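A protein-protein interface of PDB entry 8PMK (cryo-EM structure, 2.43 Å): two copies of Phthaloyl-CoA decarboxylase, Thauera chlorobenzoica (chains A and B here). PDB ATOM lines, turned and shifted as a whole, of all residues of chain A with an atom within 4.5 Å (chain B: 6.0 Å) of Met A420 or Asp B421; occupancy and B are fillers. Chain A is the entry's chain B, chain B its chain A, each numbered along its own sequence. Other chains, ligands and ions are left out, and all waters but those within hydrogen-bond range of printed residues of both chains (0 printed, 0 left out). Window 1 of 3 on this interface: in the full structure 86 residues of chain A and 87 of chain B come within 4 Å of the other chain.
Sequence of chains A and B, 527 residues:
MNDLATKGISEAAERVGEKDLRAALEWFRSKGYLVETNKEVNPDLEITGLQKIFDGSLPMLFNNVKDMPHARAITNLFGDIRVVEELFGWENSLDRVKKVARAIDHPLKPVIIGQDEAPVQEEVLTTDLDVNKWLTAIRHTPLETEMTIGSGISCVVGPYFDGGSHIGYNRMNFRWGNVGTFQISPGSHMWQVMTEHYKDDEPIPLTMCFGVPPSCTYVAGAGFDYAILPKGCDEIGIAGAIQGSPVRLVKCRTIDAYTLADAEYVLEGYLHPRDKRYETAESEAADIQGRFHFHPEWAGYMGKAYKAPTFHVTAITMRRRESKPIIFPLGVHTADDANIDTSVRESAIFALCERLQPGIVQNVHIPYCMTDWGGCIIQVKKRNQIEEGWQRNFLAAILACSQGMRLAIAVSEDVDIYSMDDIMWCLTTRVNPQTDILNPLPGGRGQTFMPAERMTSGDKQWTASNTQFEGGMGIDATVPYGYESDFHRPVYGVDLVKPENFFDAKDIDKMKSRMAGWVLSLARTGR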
ATOM      1  N   PRO A 367     -22.963  -7.944  -5.054  1.00  0.00           N
ATOM      2  CA  PRO A 367     -22.008  -8.018  -3.948  1.00  0.00           C
ATOM      3  C   PRO A 367     -20.982  -9.124  -4.093  1.00  0.00           C
ATOM      4  O   PRO A 367     -20.912  -9.815  -5.113  1.00  0.00           O
ATOM      5  CB  PRO A 367     -22.914  -8.264  -2.745  1.00  0.00           C
ATOM      6  CG  PRO A 367     -23.994  -9.037  -3.309  1.00  0.00           C
ATOM      7  CD  PRO A 367     -24.252  -8.545  -4.683  1.00  0.00           C
ATOM      8  N   CYS A 369     -21.024 -11.698  -2.092  1.00  0.00           N
ATOM      9  CA  CYS A 369     -21.718 -12.919  -1.727  1.00  0.00           C
ATOM     10  C   CYS A 369     -22.481 -13.582  -2.866  1.00  0.00           C
ATOM     11  O   CYS A 369     -22.895 -14.733  -2.713  1.00  0.00           O
ATOM     12  CB  CYS A 369     -22.651 -12.589  -0.582  1.00  0.00           C
ATOM     13  SG  CYS A 369     -24.209 -12.052  -1.167  1.00  0.00           S
ATOM     14  N   ILE A 377     -28.516  -7.908  -7.852  1.00  0.00           N
ATOM     15  CA  ILE A 377     -29.659  -7.218  -7.259  1.00  0.00           C
ATOM     16  C   ILE A 377     -29.855  -5.902  -7.994  1.00  0.00           C
ATOM     17  O   ILE A 377     -28.927  -5.093  -8.077  1.00  0.00           O
ATOM     18  CB  ILE A 377     -29.482  -6.959  -5.750  1.00  0.00           C
ATOM     19  CG1 ILE A 377     -29.205  -8.244  -4.986  1.00  0.00           C
ATOM     20  CG2 ILE A 377     -30.719  -6.333  -5.159  1.00  0.00           C
ATOM     21  CD1 ILE A 377     -28.027  -8.145  -4.139  1.00  0.00           C
ATOM     22  N   ILE A 417     -29.608  -1.314  -0.780  1.00  0.00           N
ATOM     23  CA  ILE A 417     -29.190  -2.357  -1.708  1.00  0.00           C
ATOM     24  C   ILE A 417     -27.843  -2.963  -1.319  1.00  0.00           C
ATOM     25  O   ILE A 417     -27.496  -4.048  -1.799  1.00  0.00           O
ATOM     26  CB  ILE A 417     -29.214  -1.785  -3.141  1.00  0.00           C
ATOM     27  CG1 ILE A 417     -29.530  -2.880  -4.166  1.00  0.00           C
ATOM     28  CG2 ILE A 417     -27.934  -1.015  -3.475  1.00  0.00           C
ATOM     29  CD1 ILE A 417     -29.496  -2.441  -5.607  1.00  0.00           C
ATOM     30  N   TYR A 418     -27.091  -2.327  -0.424  1.00  0.00           N
ATOM     31  CA  TYR A 418     -25.791  -2.836  -0.016  1.00  0.00           C
ATOM     32  C   TYR A 418     -25.842  -3.618   1.282  1.00  0.00           C
ATOM     33  O   TYR A 418     -24.988  -4.479   1.506  1.00  0.00           O
ATOM     34  CB  TYR A 418     -24.797  -1.683   0.125  1.00  0.00           C
ATOM     35  CG  TYR A 418     -24.827  -0.738  -1.044  1.00  0.00           C
ATOM     36  CD1 TYR A 418     -24.284  -1.115  -2.274  1.00  0.00           C
ATOM     37  CD2 TYR A 418     -25.406   0.529  -0.923  1.00  0.00           C
ATOM     38  CE1 TYR A 418     -24.308  -0.252  -3.361  1.00  0.00           C
ATOM     39  CE2 TYR A 418     -25.438   1.403  -2.004  1.00  0.00           C
ATOM     40  CZ  TYR A 418     -24.888   1.001  -3.213  1.00  0.00           C
ATOM     41  OH  TYR A 418     -24.917   1.859  -4.284  1.00  0.00           O
ATOM     42  N   SER A 419     -26.819  -3.335   2.137  1.00  0.00           N
ATOM     43  CA  SER A 419     -27.030  -4.106   3.352  1.00  0.00           C
ATOM     44  C   SER A 419     -27.694  -5.416   2.970  1.00  0.00           C
ATOM     45  O   SER A 419     -28.754  -5.419   2.340  1.00  0.00           O
ATOM     46  CB  SER A 419     -27.890  -3.329   4.338  1.00  0.00           C
ATOM     47  OG  SER A 419     -28.361  -4.189   5.351  1.00  0.00           O
ATOM     48  N   MET A 420     -27.081  -6.534   3.351  1.00  0.00           N
ATOM     49  CA  MET A 420     -27.549  -7.805   2.822  1.00  0.00           C
ATOM     50  C   MET A 420     -28.592  -8.419   3.737  1.00  0.00           C
ATOM     51  O   MET A 420     -29.293  -9.361   3.357  1.00  0.00           O
ATOM     52  CB  MET A 420     -26.358  -8.746   2.608  1.00  0.00           C
ATOM     53  CG  MET A 420     -26.528  -9.871   1.559  1.00  0.00           C
ATOM     54  SD  MET A 420     -26.840  -9.658  -0.240  1.00  0.00           S
ATOM     55  CE  MET A 420     -26.468  -7.955  -0.717  1.00  0.00           C
ATOM     56  N   ASP A 421     -28.731  -7.872   4.939  1.00  0.00           N
ATOM     57  CA  ASP A 421     -29.851  -8.243   5.784  1.00  0.00           C
ATOM     58  C   ASP A 421     -31.134  -7.579   5.314  1.00  0.00           C
ATOM     59  O   ASP A 421     -32.227  -8.096   5.559  1.00  0.00           O
ATOM     60  CB  ASP A 421     -29.540  -7.876   7.225  1.00  0.00           C
ATOM     61  CG  ASP A 421     -28.152  -8.296   7.639  1.00  0.00           C
ATOM     62  OD1 ASP A 421     -27.180  -7.761   7.070  1.00  0.00           O
ATOM     63  OD2 ASP A 421     -28.030  -9.166   8.522  1.00  0.00           O
ATOM     64  N   ASP A 422     -31.023  -6.440   4.631  1.00  0.00           N
ATOM     65  CA  ASP A 422     -32.187  -5.777   4.064  1.00  0.00           C
ATOM     66  C   ASP A 422     -32.738  -6.510   2.849  1.00  0.00           C
ATOM     67  O   ASP A 422     -33.924  -6.376   2.547  1.00  0.00           O
ATOM     68  CB  ASP A 422     -31.823  -4.341   3.693  1.00  0.00           C
ATOM     69  CG  ASP A 422     -32.849  -3.343   4.163  1.00  0.00           C
ATOM     70  OD1 ASP A 422     -34.051  -3.575   3.946  1.00  0.00           O
ATOM     71  OD2 ASP A 422     -32.456  -2.323   4.761  1.00  0.00           O
ATOM     72  N   ILE A 423     -31.906  -7.280   2.150  1.00  0.00           N
ATOM     73  CA  ILE A 423     -32.377  -8.086   1.030  1.00  0.00           C
ATOM     74  C   ILE A 423     -33.149  -9.305   1.522  1.00  0.00           C
ATOM     75  O   ILE A 423     -34.205  -9.638   0.972  1.00  0.00           O
ATOM     76  CB  ILE A 423     -31.180  -8.466   0.138  1.00  0.00           C
ATOM     77  CG1 ILE A 423     -30.411  -7.207  -0.254  1.00  0.00           C
ATOM     78  CG2 ILE A 423     -31.618  -9.219  -1.110  1.00  0.00           C
ATOM     79  CD1 ILE A 423     -31.200  -6.227  -1.094  1.00  0.00           C
ATOM     80  N   MET A 424     -32.650  -9.957   2.586  1.00  0.00           N
ATOM     81  CA  MET A 424     -33.367 -11.034   3.276  1.00  0.00           C
ATOM     82  C   MET A 424     -34.674 -10.576   3.921  1.00  0.00           C
ATOM     83  O   MET A 424     -35.603 -11.382   4.061  1.00  0.00           O
ATOM     84  CB  MET A 424     -32.480 -11.651   4.357  1.00  0.00           C
ATOM     85  CG  MET A 424     -32.843 -13.084   4.815  1.00  0.00           C
ATOM     86  SD  MET A 424     -32.587 -14.602   3.898  1.00  0.00           S
ATOM     87  CE  MET A 424     -31.004 -14.281   3.195  1.00  0.00           C
ATOM     88  N   CYS B 369     -33.303  -9.694  10.812  1.00  0.00           N
ATOM     89  CA  CYS B 369     -33.795  -9.438   9.472  1.00  0.00           C
ATOM     90  C   CYS B 369     -34.948 -10.333   9.036  1.00  0.00           C
ATOM     91  O   CYS B 369     -35.581 -10.033   8.021  1.00  0.00           O
ATOM     92  CB  CYS B 369     -32.626  -9.575   8.522  1.00  0.00           C
ATOM     93  SG  CYS B 369     -32.438 -11.226   7.980  1.00  0.00           S
ATOM     94  N   SER B 419     -23.672 -14.937   9.743  1.00  0.00           N
ATOM     95  CA  SER B 419     -23.322 -14.053   8.640  1.00  0.00           C
ATOM     96  C   SER B 419     -24.406 -14.165   7.584  1.00  0.00           C
ATOM     97  O   SER B 419     -24.698 -15.262   7.102  1.00  0.00           O
ATOM     98  CB  SER B 419     -21.964 -14.424   8.065  1.00  0.00           C
ATOM     99  OG  SER B 419     -21.782 -13.800   6.814  1.00  0.00           O
ATOM    100  N   MET B 420     -25.004 -13.035   7.215  1.00  0.00           N
ATOM    101  CA  MET B 420     -26.193 -13.111   6.381  1.00  0.00           C
ATOM    102  C   MET B 420     -25.825 -13.047   4.910  1.00  0.00           C
ATOM    103  O   MET B 420     -26.647 -13.343   4.037  1.00  0.00           O
ATOM    104  CB  MET B 420     -27.170 -11.997   6.771  1.00  0.00           C
ATOM    105  CG  MET B 420     -28.667 -12.227   6.449  1.00  0.00           C
ATOM    106  SD  MET B 420     -29.739 -13.566   7.109  1.00  0.00           S
ATOM    107  CE  MET B 420     -28.945 -14.319   8.546  1.00  0.00           C
ATOM    108  N   ASP B 421     -24.579 -12.693   4.620  1.00  0.00           N
ATOM    109  CA  ASP B 421     -24.081 -12.827   3.263  1.00  0.00           C
ATOM    110  C   ASP B 421     -23.763 -14.277   2.939  1.00  0.00           C
ATOM    111  O   ASP B 421     -23.793 -14.673   1.770  1.00  0.00           O
ATOM    112  CB  ASP B 421     -22.857 -11.945   3.086  1.00  0.00           C
ATOM    113  CG  ASP B 421     -23.058 -10.562   3.648  1.00  0.00           C
ATOM    114  OD1 ASP B 421     -23.227 -10.442   4.877  1.00  0.00           O
ATOM    115  OD2 ASP B 421     -23.059  -9.593   2.864  1.00  0.00           O
ATOM    116  N   ASP B 422     -23.468 -15.085   3.956  1.00  0.00           N
ATOM    117  CA  ASP B 422     -23.237 -16.507   3.755  1.00  0.00           C
ATOM    118  C   ASP B 422     -24.524 -17.267   3.460  1.00  0.00           C
ATOM    119  O   ASP B 422     -24.470 -18.324   2.828  1.00  0.00           O
ATOM    120  CB  ASP B 422     -22.551 -17.089   4.990  1.00  0.00           C
ATOM    121  CG  ASP B 422     -21.379 -17.968   4.641  1.00  0.00           C
ATOM    122  OD1 ASP B 422     -21.520 -18.828   3.753  1.00  0.00           O
ATOM    123  OD2 ASP B 422     -20.305 -17.796   5.250  1.00  0.00           O
ATOM    124  N   ILE B 423     -25.670 -16.754   3.899  1.00  0.00           N
ATOM    125  CA  ILE B 423     -26.951 -17.372   3.578  1.00  0.00           C
ATOM    126  C   ILE B 423     -27.340 -17.100   2.129  1.00  0.00           C
ATOM    127  O   ILE B 423     -27.806 -18.004   1.427  1.00  0.00           O
ATOM    128  CB  ILE B 423     -28.016 -16.886   4.577  1.00  0.00           C
ATOM    129  CG1 ILE B 423     -27.528 -17.123   6.004  1.00  0.00           C
ATOM    130  CG2 ILE B 423     -29.355 -17.578   4.364  1.00  0.00           C
ATOM    131  CD1 ILE B 423     -27.323 -18.578   6.364  1.00  0.00           C
ATOM    132  N   MET B 424     -27.119 -15.860   1.660  1.00  0.00           N
ATOM    133  CA  MET B 424     -27.277 -15.496   0.248  1.00  0.00           C
ATOM    134  C   MET B 424     -26.317 -16.235  -0.681  1.00  0.00           C
ATOM    135  O   MET B 424     -26.644 -16.451  -1.856  1.00  0.00           O
ATOM    136  CB  MET B 424     -27.074 -13.992   0.064  1.00  0.00           C
ATOM    137  CG  MET B 424     -27.696 -13.360  -1.204  1.00  0.00           C
ATOM    138  SD  MET B 424     -29.434 -13.047  -1.508  1.00  0.00           S
ATOM    139  CE  MET B 424     -29.935 -12.489   0.087  1.00  0.00           C
ATOM    140  N   TRP B 425     -25.138 -16.622  -0.187  1.00  0.00           N
ATOM    141  CA  TRP B 425     -24.234 -17.455  -0.970  1.00  0.00           C
ATOM    142  C   TRP B 425     -24.779 -18.869  -1.149  1.00  0.00           C
ATOM    143  O   TRP B 425     -24.564 -19.486  -2.197  1.00  0.00           O
ATOM    144  CB  TRP B 425     -22.854 -17.482  -0.312  1.00  0.00           C
ATOM    145  CG  TRP B 425     -21.860 -18.274  -1.066  1.00  0.00           C
ATOM    146  CD1 TRP B 425     -21.109 -17.851  -2.112  1.00  0.00           C
ATOM    147  CD2 TRP B 425     -21.493 -19.632  -0.827  1.00  0.00           C
ATOM    148  NE1 TRP B 425     -20.304 -18.866  -2.556  1.00  0.00           N
ATOM    149  CE2 TRP B 425     -20.521 -19.973  -1.783  1.00  0.00           C
ATOM    150  CE3 TRP B 425     -21.907 -20.601   0.094  1.00  0.00           C
ATOM    151  CZ2 TRP B 425     -19.945 -21.237  -1.840  1.00  0.00           C
ATOM    152  CZ3 TRP B 425     -21.336 -21.856   0.037  1.00  0.00           C
ATOM    153  CH2 TRP B 425     -20.368 -22.163  -0.927  1.00  0.00           C
ATOM    154  N   CYS B 426     -25.510 -19.381  -0.165  1.00  0.00           N
ATOM    155  CA  CYS B 426     -26.139 -20.684  -0.320  1.00  0.00           C
ATOM    156  C   CYS B 426     -27.385 -20.630  -1.187  1.00  0.00           C
ATOM    157  O   CYS B 426     -27.747 -21.645  -1.789  1.00  0.00           O
ATOM    158  CB  CYS B 426     -26.476 -21.265   1.044  1.00  0.00           C
ATOM    159  SG  CYS B 426     -25.022 -21.758   1.935  1.00  0.00           S
ATOM    160  N   GLY B 517     -18.586  -6.849   7.324  1.00  0.00           N
ATOM    161  CA  GLY B 517     -19.566  -7.604   6.563  1.00  0.00           C
ATOM    162  C   GLY B 517     -19.168  -9.067   6.429  1.00  0.00           C
ATOM    163  O   GLY B 517     -18.910  -9.739   7.425  1.00  0.00           O
ATOM    164  N   TRP B 518     -19.123  -9.554   5.186  1.00  0.00           N
ATOM    165  CA  TRP B 518     -18.774 -10.946   4.933  1.00  0.00           C
ATOM    166  C   TRP B 518     -17.292 -11.220   5.113  1.00  0.00           C
ATOM    167  O   TRP B 518     -16.916 -12.370   5.356  1.00  0.00           O
ATOM    168  CB  TRP B 518     -19.173 -11.354   3.517  1.00  0.00           C
ATOM    169  CG  TRP B 518     -19.392 -12.819   3.384  1.00  0.00           C
ATOM    170  CD1 TRP B 518     -19.750 -13.675   4.371  1.00  0.00           C
ATOM    171  CD2 TRP B 518     -19.234 -13.610   2.204  1.00  0.00           C
ATOM    172  NE1 TRP B 518     -19.848 -14.951   3.884  1.00  0.00           N
ATOM    173  CE2 TRP B 518     -19.532 -14.941   2.554  1.00  0.00           C
ATOM    174  CE3 TRP B 518     -18.877 -13.323   0.883  1.00  0.00           C
ATOM    175  CZ2 TRP B 518     -19.484 -15.984   1.632  1.00  0.00           C
ATOM    176  CZ3 TRP B 518     -18.820 -14.363  -0.032  1.00  0.00           C
ATOM    177  CH2 TRP B 518     -19.130 -15.675   0.346  1.00  0.00           C
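The side-chain sulfur of Cys B369 sits at hydrogen-bond distance from the side-chain sulfur of Met B420, 3.7 Å away. The side-chain carboxylate (OD2) of Asp B422 sits at hydrogen-bond distance from the indole nitrogen (NE1) of Trp B518, at 3.2 Å. SG of Cys A369 sits at hydrogen-bond distance from SD of Met A420, at 3.7 Å.
O of Asp B421 touches CB of Cys A369 (3.3 Å). Cys A369 touches Met B424 (SG to CB, 3.7 Å). Trp B425 touches Cys A369 (CA to O, 3.5 Å). Cys A369 touches Trp B518 (CA to CZ3, 3.7 Å). Cys B369 touches Asp A421. Asp A421 touches Met B420 (OD2 to CB, 3.4 Å). Cys B369 touches Met A424 (SG to CB, 3.6 Å). Met B420 touches Met A424. Met A424 touches Ile B423 (CE to CG2, 3.9 Å). Met A424 touches Met B424 (CE to CE, 3.7 Å).
Ser A419 touches none of the printed residues of chain B. Met A420 touches two residues of chain B. Printed residues of chain B within 4 Å of Asp A421: Cys B369 (3.3 Å) and Met B420 (3.4 Å). Of the printed residues of chain B, Ile A423 touches Met B424 (3.9 Å). Of the printed residues of chain A, Cys B369 touches Asp A421 (3.3 Å) and Met A424 (3.6 Å). Asp B421 touches just these residues of chain A: Cys A369 and Met A420. Of the printed residues of chain A, Met B424 touches Cys A369 (3.7 Å), Met A420 (3.9 Å), Ile A423 (3.9 Å) and Met A424 (3.7 Å). The nearest printed residue of chain A that does not touch Asp B421 is Asp A421 (5.3 Å).
Hydrophobic or aromatic side chains of chain B that line the printed part of chain A: Met B420, Ile B423, Met B424, Trp B425 and Trp B518. Hydrophobic or aromatic side chains of chain A within 4 Å of the printed part of chain B: Met A420, Ile A423 and Met A424. Among the printed residues, no Asp or Glu carboxylate lies within 4 Å of a Lys or Arg side-chain nitrogen of the other chain.
Met A420 touches Asp B421, and with the chains exchanged Asp A421 touches Met B420. Met A420 touches Met B424, and with the chains exchanged Met A424 touches Met B420. Ile A423 touches Met B424, and with the chains exchanged Met A424 touches Ile B423. Met B424 touches its own counterpart, Met A424. Of the 13 pairs that touch across the chains among the printed residues, 11 have their exchanged pair printed and touching as well.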
